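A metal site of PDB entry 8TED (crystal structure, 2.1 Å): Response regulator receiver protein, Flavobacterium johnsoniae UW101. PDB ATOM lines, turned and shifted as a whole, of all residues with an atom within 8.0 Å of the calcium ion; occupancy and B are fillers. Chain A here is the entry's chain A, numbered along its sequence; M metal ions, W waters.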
ATOM      1  N   VAL A  12      26.878 -19.285   5.850  1.00  0.00           N
ATOM      2  CA  VAL A  12      27.631 -18.857   4.632  1.00  0.00           C
ATOM      3  C   VAL A  12      27.961 -17.387   4.793  1.00  0.00           C
ATOM      4  O   VAL A  12      27.003 -16.568   4.856  1.00  0.00           O
ATOM      5  CB  VAL A  12      26.815 -19.048   3.333  1.00  0.00           C
ATOM      6  CG1 VAL A  12      27.671 -18.893   2.094  1.00  0.00           C
ATOM      7  CG2 VAL A  12      26.084 -20.367   3.325  1.00  0.00           C
ATOM      8  N   ASP A  13      29.262 -17.076   4.846  1.00  0.00           N
ATOM      9  CA  ASP A  13      29.803 -15.703   4.985  1.00  0.00           C
ATOM     10  C   ASP A  13      31.263 -15.735   4.551  1.00  0.00           C
ATOM     11  O   ASP A  13      31.963 -16.674   4.931  1.00  0.00           O
ATOM     12  CB  ASP A  13      29.646 -15.181   6.418  1.00  0.00           C
ATOM     13  CG  ASP A  13      29.814 -13.677   6.536  1.00  0.00           C
ATOM     14  OD1 ASP A  13      30.801 -13.139   5.955  1.00  0.00           O
ATOM     15  OD2 ASP A  13      28.937 -13.058   7.179  1.00  0.00           O
ATOM     16  N   ASP A  14      31.706 -14.762   3.748  1.00  0.00           N
ATOM     17  CA  ASP A  14      33.109 -14.756   3.237  1.00  0.00           C
ATOM     18  C   ASP A  14      34.054 -14.500   4.410  1.00  0.00           C
ATOM     19  O   ASP A  14      35.230 -14.875   4.280  1.00  0.00           O
ATOM     20  CB  ASP A  14      33.300 -13.762   2.096  1.00  0.00           C
ATOM     21  CG  ASP A  14      33.003 -12.328   2.483  1.00  0.00           C
ATOM     22  OD1 ASP A  14      33.944 -11.616   2.832  1.00  0.00           O
ATOM     23  OD2 ASP A  14      31.836 -11.943   2.506  1.00  0.00           O
ATOM     24  N   GLU A  15      33.543 -13.935   5.510  1.00  0.00           N
ATOM     25  CA  GLU A  15      34.333 -13.605   6.732  1.00  0.00           C
ATOM     26  C   GLU A  15      33.841 -14.439   7.909  1.00  0.00           C
ATOM     27  O   GLU A  15      33.801 -13.927   9.014  1.00  0.00           O
ATOM     28  CB  GLU A  15      34.200 -12.105   7.003  1.00  0.00           C
ATOM     29  CG  GLU A  15      34.829 -11.243   5.936  1.00  0.00           C
ATOM     30  CD  GLU A  15      34.582  -9.752   6.067  1.00  0.00           C
ATOM     31  OE1 GLU A  15      33.544  -9.351   6.616  1.00  0.00           O
ATOM     32  OE2 GLU A  15      35.436  -8.990   5.589  1.00  0.00           O
ATOM     33  N   ILE A  16      33.536 -15.716   7.688  1.00  0.00           N
ATOM     34  CA  ILE A  16      33.011 -16.638   8.744  1.00  0.00           C
ATOM     35  C   ILE A  16      34.078 -16.791   9.848  1.00  0.00           C
ATOM     36  O   ILE A  16      33.687 -17.144  10.975  1.00  0.00           O
ATOM     37  CB  ILE A  16      32.497 -17.966   8.118  1.00  0.00           C
ATOM     38  CG1 ILE A  16      31.613 -18.781   9.054  1.00  0.00           C
ATOM     39  CG2 ILE A  16      33.614 -18.834   7.551  1.00  0.00           C
ATOM     40  CD1 ILE A  16      30.583 -17.974   9.812  1.00  0.00           C
ATOM     41  N   ASN A  37      32.525 -20.493   3.254  1.00  0.00           N
ATOM     42  CA  ASN A  37      32.993 -19.108   2.966  1.00  0.00           C
ATOM     43  C   ASN A  37      32.500 -18.660   1.596  1.00  0.00           C
ATOM     44  O   ASN A  37      32.804 -17.499   1.244  1.00  0.00           O
ATOM     45  CB  ASN A  37      34.493 -18.947   3.175  1.00  0.00           C
ATOM     46  CG  ASN A  37      35.329 -19.766   2.207  1.00  0.00           C
ATOM     47  OD1 ASN A  37      34.861 -20.144   1.145  1.00  0.00           O
ATOM     48  ND2 ASN A  37      36.554 -20.045   2.583  1.00  0.00           N
ATOM     49  N   ASP A  57      25.192 -14.259   4.324  1.00  0.00           N
ATOM     50  CA  ASP A  57      25.624 -12.854   4.116  1.00  0.00           C
ATOM     51  C   ASP A  57      25.142 -12.407   2.737  1.00  0.00           C
ATOM     52  O   ASP A  57      25.040 -13.276   1.865  1.00  0.00           O
ATOM     53  CB  ASP A  57      27.139 -12.771   4.292  1.00  0.00           C
ATOM     54  CG  ASP A  57      27.727 -11.368   4.161  1.00  0.00           C
ATOM     55  OD1 ASP A  57      27.019 -10.347   4.416  1.00  0.00           O
ATOM     56  OD2 ASP A  57      28.905 -11.327   3.842  1.00  0.00           O
ATOM     57  N   GLU A  58      24.859 -11.126   2.516  1.00  0.00           N
ATOM     58  CA  GLU A  58      24.481 -10.634   1.166  1.00  0.00           C
ATOM     59  C   GLU A  58      25.751 -10.427   0.323  1.00  0.00           C
ATOM     60  O   GLU A  58      25.826 -11.020  -0.744  1.00  0.00           O
ATOM     61  CB  GLU A  58      23.624  -9.374   1.183  1.00  0.00           C
ATOM     62  CG  GLU A  58      23.479  -8.724  -0.220  1.00  0.00           C
ATOM     63  CD  GLU A  58      22.994  -9.602  -1.377  1.00  0.00           C
ATOM     64  OE1 GLU A  58      22.717 -10.805  -1.165  1.00  0.00           O
ATOM     65  OE2 GLU A  58      22.831  -9.076  -2.488  1.00  0.00           O
ATOM     66  N   ASN A  59      26.701  -9.608   0.760  1.00  0.00           N
ATOM     67  CA  ASN A  59      27.847  -9.190  -0.109  1.00  0.00           C
ATOM     68  C   ASN A  59      28.972 -10.214   0.076  1.00  0.00           C
ATOM     69  O   ASN A  59      29.524 -10.290   1.195  1.00  0.00           O
ATOM     70  CB  ASN A  59      28.294  -7.734   0.101  1.00  0.00           C
ATOM     71  CG  ASN A  59      27.382  -6.742  -0.600  1.00  0.00           C
ATOM     72  OD1 ASN A  59      26.924  -6.976  -1.715  1.00  0.00           O
ATOM     73  ND2 ASN A  59      27.116  -5.618   0.048  1.00  0.00           N
ATOM     74  N   MET A  60      29.239 -10.977  -0.983  1.00  0.00           N
ATOM     75  CA  MET A  60      30.319 -11.994  -1.059  1.00  0.00           C
ATOM     76  C   MET A  60      30.957 -11.957  -2.463  1.00  0.00           C
ATOM     77  O   MET A  60      30.315 -11.597  -3.448  1.00  0.00           O
ATOM     78  CB  MET A  60      29.767 -13.385  -0.752  1.00  0.00           C
ATOM     79  CG  MET A  60      29.331 -13.593   0.696  1.00  0.00           C
ATOM     80  SD  MET A  60      28.823 -15.343   1.084  1.00  0.00           S
ATOM     81  CE  MET A  60      27.302 -15.454   0.159  1.00  0.00           C
ATOM     82  N   PRO A  61      32.265 -12.255  -2.576  1.00  0.00           N
ATOM     83  CA  PRO A  61      33.003 -12.067  -3.832  1.00  0.00           C
ATOM     84  C   PRO A  61      32.403 -12.804  -5.036  1.00  0.00           C
ATOM     85  O   PRO A  61      32.278 -12.204  -6.089  1.00  0.00           O
ATOM     86  CB  PRO A  61      34.392 -12.658  -3.547  1.00  0.00           C
ATOM     87  CG  PRO A  61      34.522 -12.613  -2.044  1.00  0.00           C
ATOM     88  CD  PRO A  61      33.108 -12.743  -1.492  1.00  0.00           C
ATOM     89  N   ILE A  84      22.058 -12.374   7.256  1.00  0.00           N
ATOM     90  CA  ILE A  84      22.869 -11.717   8.332  1.00  0.00           C
ATOM     91  C   ILE A  84      24.015 -10.970   7.656  1.00  0.00           C
ATOM     92  O   ILE A  84      24.968 -11.653   7.176  1.00  0.00           O
ATOM     93  CB  ILE A  84      23.378 -12.745   9.359  1.00  0.00           C
ATOM     94  CG1 ILE A  84      22.239 -13.587   9.933  1.00  0.00           C
ATOM     95  CG2 ILE A  84      24.181 -12.060  10.457  1.00  0.00           C
ATOM     96  CD1 ILE A  84      22.655 -14.574  11.033  1.00  0.00           C
ATOM     97  N   THR A  85      23.949  -9.638   7.625  1.00  0.00           N
ATOM     98  CA  THR A  85      24.670  -8.790   6.647  1.00  0.00           C
ATOM     99  C   THR A  85      24.876  -7.364   7.185  1.00  0.00           C
ATOM    100  O   THR A  85      24.062  -6.911   8.018  1.00  0.00           O
ATOM    101  CB  THR A  85      23.860  -8.739   5.350  1.00  0.00           C
ATOM    102  OG1 THR A  85      24.507  -7.922   4.381  1.00  0.00           O
ATOM    103  CG2 THR A  85      22.482  -8.143   5.540  1.00  0.00           C
ATOM    104  N   LYS A  86      25.890  -6.665   6.655  1.00  0.00           N
ATOM    105  CA  LYS A  86      26.184  -5.235   6.991  1.00  0.00           C
ATOM    106  C   LYS A  86      25.214  -4.355   6.209  1.00  0.00           C
ATOM    107  O   LYS A  86      25.008  -3.236   6.631  1.00  0.00           O
ATOM    108  CB  LYS A  86      27.638  -4.847   6.713  1.00  0.00           C
ATOM    109  CG  LYS A  86      28.703  -5.459   7.606  1.00  0.00           C
ATOM    110  CD  LYS A  86      28.909  -4.752   8.957  1.00  0.00           C
ATOM    111  CE  LYS A  86      29.925  -5.435   9.859  1.00  0.00           C
ATOM    112  NZ  LYS A  86      29.881  -4.957  11.268  1.00  0.00           N
ATOM    113  N   SER A  87      24.590  -4.853   5.137  1.00  0.00           N
ATOM    114  CA  SER A  87      23.776  -4.052   4.189  1.00  0.00           C
ATOM    115  C   SER A  87      22.553  -3.459   4.892  1.00  0.00           C
ATOM    116  O   SER A  87      21.788  -4.215   5.512  1.00  0.00           O
ATOM    117  CB  SER A  87      23.355  -4.918   3.021  1.00  0.00           C
ATOM    118  OG  SER A  87      24.427  -5.754   2.605  1.00  0.00           O
ATOM    119  N   LYS A 107      24.228  -6.521  10.787  1.00  0.00           N
ATOM    120  CA  LYS A 107      25.513  -6.542  11.523  1.00  0.00           C
ATOM    121  C   LYS A 107      25.863  -5.128  11.983  1.00  0.00           C
ATOM    122  O   LYS A 107      25.522  -4.172  11.279  1.00  0.00           O
ATOM    123  CB  LYS A 107      26.651  -7.070  10.644  1.00  0.00           C
ATOM    124  CG  LYS A 107      26.650  -8.547  10.345  1.00  0.00           C
ATOM    125  CD  LYS A 107      27.849  -8.937   9.504  1.00  0.00           C
ATOM    126  CE  LYS A 107      27.805 -10.394   9.088  1.00  0.00           C
ATOM    127  NZ  LYS A 107      28.958 -10.702   8.216  1.00  0.00           N
HETATM  128 CA    CA M   1      30.708 -10.126   3.012  1.00  0.00          CA
HETATM  129  O   HOH W   1      29.974  -7.786   3.572  1.00  0.00           O
HETATM  130  O   HOH W   2      32.892  -8.839   2.836  1.00  0.00           O
HETATM  131  O   HOH W   3      31.258 -10.661   5.170  1.00  0.00           O
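OD1 of Asp 57 is in hydrogen-bond range of OG1 of Thr 85 (3.5 Å). N of Asp 57 is in hydrogen-bond range of O of Val 12 (3.0 Å).
Of the 16 residues printed, 3 come within 4 Å of the calcium ion. The nearest printed residue that does not touch the calcium ion is Asp 13 (4.2 Å).
The calcium ion is bound by O of Asn 59 (2.2 Å), OD2 of Asp 14 (2.2 Å), water W3 (2.3 Å), OD2 of Asp 57 (2.3 Å), water W1 (2.5 Å) and water W2 (2.5 Å).
Water W3 bridges the side-chain carboxylate of Asp 13 (2.6 Å) and the side-chain carboxylate of Glu 15 (3.0 Å).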
